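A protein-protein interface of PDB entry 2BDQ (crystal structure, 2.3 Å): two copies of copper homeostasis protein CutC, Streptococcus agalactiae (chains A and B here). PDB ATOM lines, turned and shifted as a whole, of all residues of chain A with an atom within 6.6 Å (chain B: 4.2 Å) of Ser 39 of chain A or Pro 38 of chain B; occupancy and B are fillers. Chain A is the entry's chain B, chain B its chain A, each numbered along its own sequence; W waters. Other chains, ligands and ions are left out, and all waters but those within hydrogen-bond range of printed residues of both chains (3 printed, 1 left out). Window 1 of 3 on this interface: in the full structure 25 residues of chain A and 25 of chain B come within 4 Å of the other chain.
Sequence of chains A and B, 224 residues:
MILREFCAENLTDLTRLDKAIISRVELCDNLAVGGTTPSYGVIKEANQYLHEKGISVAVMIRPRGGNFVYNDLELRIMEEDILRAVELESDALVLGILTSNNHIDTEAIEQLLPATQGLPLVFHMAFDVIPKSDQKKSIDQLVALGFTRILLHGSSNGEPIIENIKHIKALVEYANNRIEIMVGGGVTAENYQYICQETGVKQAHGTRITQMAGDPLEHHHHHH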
ATOM      1  N   ASN A  10      16.721   2.659  15.904  1.00  0.00           N
ATOM      2  CA  ASN A  10      16.290   1.268  15.938  1.00  0.00           C
ATOM      3  C   ASN A  10      17.423   0.413  16.506  1.00  0.00           C
ATOM      4  O   ASN A  10      18.340   0.949  17.123  1.00  0.00           O
ATOM      5  CB  ASN A  10      15.895   0.843  14.536  1.00  0.00           C
ATOM      6  CG  ASN A  10      14.800   1.721  13.979  1.00  0.00           C
ATOM      7  OD1 ASN A  10      14.710   1.942  12.772  1.00  0.00           O
ATOM      8  ND2 ASN A  10      13.951   2.230  14.867  1.00  0.00           N
ATOM      9  N   LEU A  27      17.426   5.658  22.511  1.00  0.00           N
ATOM     10  CA  LEU A  27      16.679   4.932  21.500  1.00  0.00           C
ATOM     11  C   LEU A  27      15.651   5.812  20.783  1.00  0.00           C
ATOM     12  O   LEU A  27      14.763   6.399  21.406  1.00  0.00           O
ATOM     13  CB  LEU A  27      15.956   3.738  22.147  1.00  0.00           C
ATOM     14  CG  LEU A  27      15.604   2.482  21.330  1.00  0.00           C
ATOM     15  CD1 LEU A  27      14.402   1.760  21.954  1.00  0.00           C
ATOM     16  CD2 LEU A  27      15.276   2.866  19.915  1.00  0.00           C
ATOM     17  N   ASP A  29      14.054   6.797  16.391  1.00  0.00           N
ATOM     18  CA  ASP A  29      14.027   6.419  14.988  1.00  0.00           C
ATOM     19  C   ASP A  29      14.150   7.729  14.237  1.00  0.00           C
ATOM     20  O   ASP A  29      14.272   8.787  14.862  1.00  0.00           O
ATOM     21  CB  ASP A  29      12.707   5.711  14.653  1.00  0.00           C
ATOM     22  CG  ASP A  29      12.667   5.175  13.230  1.00  0.00           C
ATOM     23  OD1 ASP A  29      13.727   4.831  12.671  1.00  0.00           O
ATOM     24  OD2 ASP A  29      11.563   5.073  12.668  1.00  0.00           O
ATOM     25  N   THR A  37      10.079   9.169  18.274  1.00  0.00           N
ATOM     26  CA  THR A  37       9.742   8.014  19.077  1.00  0.00           C
ATOM     27  C   THR A  37       9.727   6.786  18.178  1.00  0.00           C
ATOM     28  O   THR A  37       9.070   6.775  17.138  1.00  0.00           O
ATOM     29  CB  THR A  37       8.367   8.174  19.713  1.00  0.00           C
ATOM     30  OG1 THR A  37       8.333   9.395  20.468  1.00  0.00           O
ATOM     31  CG2 THR A  37       8.072   6.994  20.627  1.00  0.00           C
ATOM     32  N   PRO A  38      10.476   5.740  18.560  1.00  0.00           N
ATOM     33  CA  PRO A  38      10.549   4.498  17.785  1.00  0.00           C
ATOM     34  C   PRO A  38       9.268   3.681  17.948  1.00  0.00           C
ATOM     35  O   PRO A  38       8.452   3.961  18.829  1.00  0.00           O
ATOM     36  CB  PRO A  38      11.772   3.802  18.374  1.00  0.00           C
ATOM     37  CG  PRO A  38      11.750   4.248  19.797  1.00  0.00           C
ATOM     38  CD  PRO A  38      11.422   5.713  19.691  1.00  0.00           C
ATOM     39  N   SER A  39       9.090   2.672  17.106  1.00  0.00           N
ATOM     40  CA  SER A  39       7.888   1.844  17.180  1.00  0.00           C
ATOM     41  C   SER A  39       7.824   1.083  18.498  1.00  0.00           C
ATOM     42  O   SER A  39       8.823   0.968  19.204  1.00  0.00           O
ATOM     43  CB  SER A  39       7.848   0.850  16.014  1.00  0.00           C
ATOM     44  OG  SER A  39       8.791  -0.187  16.201  1.00  0.00           O
ATOM     45  N   TYR A  40       6.644   0.560  18.823  1.00  0.00           N
ATOM     46  CA  TYR A  40       6.465  -0.196  20.054  1.00  0.00           C
ATOM     47  C   TYR A  40       7.378  -1.416  20.046  1.00  0.00           C
ATOM     48  O   TYR A  40       8.061  -1.692  21.029  1.00  0.00           O
ATOM     49  CB  TYR A  40       5.011  -0.643  20.188  1.00  0.00           C
ATOM     50  CG  TYR A  40       4.676  -1.340  21.490  1.00  0.00           C
ATOM     51  CD1 TYR A  40       4.169  -0.628  22.577  1.00  0.00           C
ATOM     52  CD2 TYR A  40       4.796  -2.720  21.613  1.00  0.00           C
ATOM     53  CE1 TYR A  40       3.780  -1.280  23.748  1.00  0.00           C
ATOM     54  CE2 TYR A  40       4.413  -3.379  22.776  1.00  0.00           C
ATOM     55  CZ  TYR A  40       3.907  -2.663  23.835  1.00  0.00           C
ATOM     56  OH  TYR A  40       3.524  -3.333  24.979  1.00  0.00           O
ATOM     57  N   GLY A  41       7.383  -2.144  18.931  1.00  0.00           N
ATOM     58  CA  GLY A  41       8.226  -3.321  18.811  1.00  0.00           C
ATOM     59  C   GLY A  41       9.693  -3.027  19.086  1.00  0.00           C
ATOM     60  O   GLY A  41      10.366  -3.785  19.787  1.00  0.00           O
ATOM     61  N   VAL A  42      10.189  -1.920  18.543  1.00  0.00           N
ATOM     62  CA  VAL A  42      11.580  -1.540  18.732  1.00  0.00           C
ATOM     63  C   VAL A  42      11.890  -1.236  20.193  1.00  0.00           C
ATOM     64  O   VAL A  42      12.932  -1.629  20.704  1.00  0.00           O
ATOM     65  CB  VAL A  42      11.944  -0.306  17.849  1.00  0.00           C
ATOM     66  CG1 VAL A  42      13.253   0.329  18.333  1.00  0.00           C
ATOM     67  CG2 VAL A  42      12.093  -0.740  16.394  1.00  0.00           C
ATOM     68  N   ILE A  43      10.984  -0.540  20.869  1.00  0.00           N
ATOM     69  CA  ILE A  43      11.195  -0.195  22.272  1.00  0.00           C
ATOM     70  C   ILE A  43      11.247  -1.448  23.158  1.00  0.00           C
ATOM     71  O   ILE A  43      12.149  -1.599  23.996  1.00  0.00           O
ATOM     72  CB  ILE A  43      10.076   0.751  22.786  1.00  0.00           C
ATOM     73  CG1 ILE A  43      10.143   2.081  22.043  1.00  0.00           C
ATOM     74  CG2 ILE A  43      10.233   0.984  24.294  1.00  0.00           C
ATOM     75  CD1 ILE A  43       9.015   3.038  22.401  1.00  0.00           C
ATOM     76  N   LYS A  44      10.281  -2.340  22.969  1.00  0.00           N
ATOM     77  CA  LYS A  44      10.215  -3.565  23.744  1.00  0.00           C
ATOM     78  C   LYS A  44      11.443  -4.442  23.543  1.00  0.00           C
ATOM     79  O   LYS A  44      12.085  -4.864  24.511  1.00  0.00           O
ATOM     80  CB  LYS A  44       8.949  -4.344  23.376  1.00  0.00           C
ATOM     81  CG  LYS A  44       8.846  -5.747  23.967  1.00  0.00           C
ATOM     82  CD  LYS A  44       7.554  -6.407  23.484  1.00  0.00           C
ATOM     83  CE  LYS A  44       7.459  -7.865  23.894  1.00  0.00           C
ATOM     84  NZ  LYS A  44       7.486  -8.004  25.367  1.00  0.00           N
ATOM     85  N   LEU A  88       7.118  -0.698  29.193  1.00  0.00           N
ATOM     86  CA  LEU A  88       8.121  -1.529  28.532  1.00  0.00           C
ATOM     87  C   LEU A  88       9.464  -1.471  29.262  1.00  0.00           C
ATOM     88  O   LEU A  88      10.499  -1.882  28.729  1.00  0.00           O
ATOM     89  CB  LEU A  88       8.293  -1.105  27.063  1.00  0.00           C
ATOM     90  CG  LEU A  88       7.087  -1.447  26.179  1.00  0.00           C
ATOM     91  CD1 LEU A  88       7.253  -0.874  24.784  1.00  0.00           C
ATOM     92  CD2 LEU A  88       6.927  -2.971  26.134  1.00  0.00           C
ATOM     93  N   LEU B  27       0.450   4.801   6.699  1.00  0.00           N
ATOM     94  CA  LEU B  27       1.040   5.407   7.882  1.00  0.00           C
ATOM     95  C   LEU B  27       2.404   4.808   8.241  1.00  0.00           C
ATOM     96  O   LEU B  27       2.535   3.608   8.458  1.00  0.00           O
ATOM     97  CB  LEU B  27       0.083   5.246   9.076  1.00  0.00           C
ATOM     98  CG  LEU B  27       0.111   6.238  10.250  1.00  0.00           C
ATOM     99  CD1 LEU B  27      -0.402   5.572  11.518  1.00  0.00           C
ATOM    100  CD2 LEU B  27       1.523   6.722  10.478  1.00  0.00           C
ATOM    101  N   CYS B  28       3.423   5.653   8.290  1.00  0.00           N
ATOM    102  CA  CYS B  28       4.749   5.208   8.678  1.00  0.00           C
ATOM    103  C   CYS B  28       5.555   6.392   9.183  1.00  0.00           C
ATOM    104  O   CYS B  28       5.036   7.505   9.306  1.00  0.00           O
ATOM    105  CB  CYS B  28       5.471   4.504   7.516  1.00  0.00           C
ATOM    106  SG  CYS B  28       5.241   5.184   5.854  1.00  0.00           S
ATOM    107  N   ASP B  29       6.811   6.149   9.527  1.00  0.00           N
ATOM    108  CA  ASP B  29       7.668   7.222   9.987  1.00  0.00           C
ATOM    109  C   ASP B  29       8.957   7.052   9.196  1.00  0.00           C
ATOM    110  O   ASP B  29       9.050   6.169   8.339  1.00  0.00           O
ATOM    111  CB  ASP B  29       7.915   7.092  11.497  1.00  0.00           C
ATOM    112  CG  ASP B  29       8.721   8.249  12.065  1.00  0.00           C
ATOM    113  OD1 ASP B  29       8.641   9.371  11.528  1.00  0.00           O
ATOM    114  OD2 ASP B  29       9.430   8.049  13.066  1.00  0.00           O
ATOM    115  N   THR B  36       9.261   3.409   8.066  1.00  0.00           N
ATOM    116  CA  THR B  36       9.323   2.360   9.073  1.00  0.00           C
ATOM    117  C   THR B  36       8.040   2.392   9.890  1.00  0.00           C
ATOM    118  O   THR B  36       7.166   3.236   9.679  1.00  0.00           O
ATOM    119  CB  THR B  36      10.508   2.543  10.047  1.00  0.00           C
ATOM    120  OG1 THR B  36      10.367   3.780  10.754  1.00  0.00           O
ATOM    121  CG2 THR B  36      11.833   2.527   9.303  1.00  0.00           C
ATOM    122  N   THR B  37       7.931   1.464  10.826  1.00  0.00           N
ATOM    123  CA  THR B  37       6.764   1.396  11.676  1.00  0.00           C
ATOM    124  C   THR B  37       6.756   2.611  12.588  1.00  0.00           C
ATOM    125  O   THR B  37       7.746   2.885  13.267  1.00  0.00           O
ATOM    126  CB  THR B  37       6.798   0.143  12.548  1.00  0.00           C
ATOM    127  OG1 THR B  37       6.914  -1.014  11.711  1.00  0.00           O
ATOM    128  CG2 THR B  37       5.529   0.049  13.384  1.00  0.00           C
ATOM    129  N   PRO B  38       5.645   3.367  12.599  1.00  0.00           N
ATOM    130  CA  PRO B  38       5.502   4.564  13.436  1.00  0.00           C
ATOM    131  C   PRO B  38       5.308   4.186  14.908  1.00  0.00           C
ATOM    132  O   PRO B  38       5.057   3.025  15.229  1.00  0.00           O
ATOM    133  CB  PRO B  38       4.275   5.260  12.839  1.00  0.00           C
ATOM    134  CG  PRO B  38       3.447   4.107  12.352  1.00  0.00           C
ATOM    135  CD  PRO B  38       4.469   3.189  11.723  1.00  0.00           C
ATOM    136  N   SER B  39       5.429   5.165  15.801  1.00  0.00           N
ATOM    137  CA  SER B  39       5.271   4.907  17.227  1.00  0.00           C
ATOM    138  C   SER B  39       3.842   4.464  17.551  1.00  0.00           C
ATOM    139  O   SER B  39       2.919   4.649  16.746  1.00  0.00           O
ATOM    140  CB  SER B  39       5.614   6.161  18.034  1.00  0.00           C
ATOM    141  OG  SER B  39       4.580   7.137  17.930  1.00  0.00           O
ATOM    142  N   TYR B  40       3.661   3.874  18.730  1.00  0.00           N
ATOM    143  CA  TYR B  40       2.343   3.409  19.155  1.00  0.00           C
ATOM    144  C   TYR B  40       1.367   4.581  19.212  1.00  0.00           C
ATOM    145  O   TYR B  40       0.240   4.485  18.742  1.00  0.00           O
ATOM    146  CB  TYR B  40       2.436   2.755  20.535  1.00  0.00           C
ATOM    147  CG  TYR B  40       1.150   2.120  21.028  1.00  0.00           C
ATOM    148  CD1 TYR B  40       0.891   0.769  20.816  1.00  0.00           C
ATOM    149  CD2 TYR B  40       0.223   2.859  21.758  1.00  0.00           C
ATOM    150  CE1 TYR B  40      -0.264   0.161  21.332  1.00  0.00           C
ATOM    151  CE2 TYR B  40      -0.928   2.273  22.277  1.00  0.00           C
ATOM    152  CZ  TYR B  40      -1.163   0.925  22.066  1.00  0.00           C
ATOM    153  OH  TYR B  40      -2.278   0.337  22.600  1.00  0.00           O
ATOM    154  N   VAL B  42       1.380   7.377  17.563  1.00  0.00           N
ATOM    155  CA  VAL B  42       1.028   7.837  16.229  1.00  0.00           C
ATOM    156  C   VAL B  42      -0.016   6.921  15.590  1.00  0.00           C
ATOM    157  O   VAL B  42      -0.963   7.398  14.973  1.00  0.00           O
ATOM    158  CB  VAL B  42       2.282   7.914  15.317  1.00  0.00           C
ATOM    159  CG1 VAL B  42       1.867   7.979  13.850  1.00  0.00           C
ATOM    160  CG2 VAL B  42       3.094   9.149  15.662  1.00  0.00           C
ATOM    161  N   ILE B  43       0.151   5.612  15.741  1.00  0.00           N
ATOM    162  CA  ILE B  43      -0.796   4.656  15.158  1.00  0.00           C
ATOM    163  C   ILE B  43      -2.197   4.816  15.767  1.00  0.00           C
ATOM    164  O   ILE B  43      -3.200   4.903  15.049  1.00  0.00           O
ATOM    165  CB  ILE B  43      -0.307   3.194  15.362  1.00  0.00           C
ATOM    166  CG1 ILE B  43       1.005   2.972  14.596  1.00  0.00           C
ATOM    167  CG2 ILE B  43      -1.357   2.207  14.855  1.00  0.00           C
ATOM    168  CD1 ILE B  43       1.642   1.606  14.845  1.00  0.00           C
ATOM    169  N   MET B  60       2.590   0.693   8.182  1.00  0.00           N
ATOM    170  CA  MET B  60       3.869   0.135   7.760  1.00  0.00           C
ATOM    171  C   MET B  60       4.483  -0.748   8.839  1.00  0.00           C
ATOM    172  O   MET B  60       4.590  -0.356  10.003  1.00  0.00           O
ATOM    173  CB  MET B  60       4.858   1.257   7.414  1.00  0.00           C
ATOM    174  CG  MET B  60       5.205   1.348   5.939  1.00  0.00           C
ATOM    175  SD  MET B  60       6.346  -0.127   5.403  1.00  0.00           S
ATOM    176  CE  MET B  60       7.526   0.825   4.203  1.00  0.00           C
ATOM    177  N   ASP B  81       4.869  -5.439  16.526  1.00  0.00           N
ATOM    178  CA  ASP B  81       4.255  -4.249  15.956  1.00  0.00           C
ATOM    179  C   ASP B  81       2.952  -4.565  15.235  1.00  0.00           C
ATOM    180  O   ASP B  81       2.054  -3.719  15.166  1.00  0.00           O
ATOM    181  CB  ASP B  81       5.242  -3.511  15.043  1.00  0.00           C
ATOM    182  CG  ASP B  81       6.234  -2.672  15.840  1.00  0.00           C
ATOM    183  OD1 ASP B  81       5.786  -2.003  16.806  1.00  0.00           O
ATOM    184  OD2 ASP B  81       7.443  -2.662  15.513  1.00  0.00           O
HETATM  185  O   HOH W   1      10.741   2.338  14.694  1.00  0.00           O
HETATM  186  O   HOH W   2       4.240   1.110  17.246  1.00  0.00           O
HETATM  187  O   HOH W   3       5.877   3.359  20.269  1.00  0.00           O
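The side-chain hydroxyl of Thr 36 of chain B sits at hydrogen-bond distance from the side-chain carboxylate of Asp 29 of chain A, 2.6 Å away. The side-chain carboxylate (OD2) of Asp 81 of chain B sits at hydrogen-bond distance from the side-chain hydroxyl (OG) of Ser 39 of chain A, 2.9 Å away. The backbone NH of Tyr 40 of chain A sits at hydrogen-bond distance from the side-chain carboxylate of Asp 81 of chain B (3.4 Å). OD1 of Asp 81 of chain B sits at hydrogen-bond distance from N of Gly 41 of chain A, at 2.7 Å.
The backbone NH (N) of Thr 36 of chain B sits at hydrogen-bond distance from the backbone carbonyl oxygen (O) of Asp 29 of chain B (2.8 Å). The side-chain hydroxyl (OG1) of Thr 37 of chain B is in hydrogen-bond range of the backbone carbonyl oxygen (O) of Met 60 of chain B, at 3.0 Å. N of Val 42 of chain B is in hydrogen-bond range of OG of Ser 39 of chain B (3.2 Å). OD1 of Asp 29 of chain A sits close to OD1 of Asn 10 of chain A, at 3.1 Å. The backbone NH of Val 42 of chain A lies within hydrogen-bond range of the side-chain hydroxyl of Ser 39 of chain A, 3.2 Å away.
Among the printed residues, merely in contact across the chains: Ser 39 of chain A with Thr 37 of chain B, Thr 37 of chain A with Ser 39 of chain B, Ser 39 of chain A with Pro 38 of chain B, Pro 38 of chain A with Ser 39 of chain B, Asp 29 of chain A with Asp 29 of chain B and Tyr 40 of chain A with Tyr 40 of chain B.
Printed residues of chain B within 4 Å of Asp 29 of chain A: Asp 29 (3.7 Å) and Thr 36 (2.6 Å). Of the printed residues of chain B, Thr 37 of chain A touches Ser 39 (3.6 Å). Ser 39 of chain A touches just these residues of chain B: Thr 37, Pro 38 and Asp 81. Of the printed residues of chain B, Tyr 40 of chain A touches Tyr 40 (3.97 Å) and Asp 81 (3.4 Å). Of the printed residues of chain A, Thr 36 of chain B touches Asp 29 (2.6 Å). Printed residues of chain A within 4 Å of Thr 37 of chain B: Ser 39. Of the printed residues of chain A, Pro 38 of chain B touches Ser 39. Met 60 of chain B touches none of the printed residues of chain A. The nearest residue of chain B that does not touch Ser 39 of chain A is Ser 39 of chain B (4.03 Å). The nearest residue of chain A that does not touch Pro 38 of chain B is Tyr 40 of chain A (4.6 Å).
Of the 12 printed residues of chain B, 7 touch a printed residue of chain A. Printed residues of chain B that touch a printed residue of chain A: Asp 29, Thr 36, Thr 37, Pro 38, Ser 39, Tyr 40 and Asp 81. Hydrophobic or aromatic side chains of chain B within 4 Å of the printed part of chain A: Tyr 40. Hydrophobic or aromatic side chains of chain A that line the printed part of chain B: Tyr 40. Among the printed residues, no Asp or Glu carboxylate lies within 4 Å of a Lys or Arg side-chain nitrogen of the other chain.
Asp 29 of chain B touches its own counterpart, Asp 29 of chain A. Thr 37 of chain A touches Ser 39 of chain B, and with the chains exchanged Ser 39 of chain A touches Thr 37 of chain B. Pro 38 of chain A touches Ser 39 of chain B, and with the chains exchanged Ser 39 of chain A touches Pro 38 of chain B. Tyr 40 of chain B touches its own counterpart, Tyr 40 of chain A. Positions printed for both chains: 27, 29, 37, 38, 39, 40, 42 and 43. Of the 10 pairs that touch across the chains among the printed residues, 6 have their exchanged pair printed and touching as well.
Water W3 lies within hydrogen-bond range of the backbone NH (N) of Tyr 40 of chain B (2.7 Å), the backbone carbonyl oxygen (O) of Pro 38 of chain A (3.0 Å) and the backbone NH (N) of Tyr 40 of chain A (3.2 Å). Water W2 lies within hydrogen-bond range of the backbone carbonyl oxygen (O) of Pro 38 of chain B (2.9 Å), the backbone NH (N) of Tyr 40 of chain A (2.9 Å) and the backbone NH (N) of Tyr 40 of chain B (3.2 Å). Water W1 lies within hydrogen-bond range of the backbone NH of Ser 39 of chain A, the side-chain amide nitrogen of Asn 10 of chain A and the backbone carbonyl oxygen of Thr 37 of chain B.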
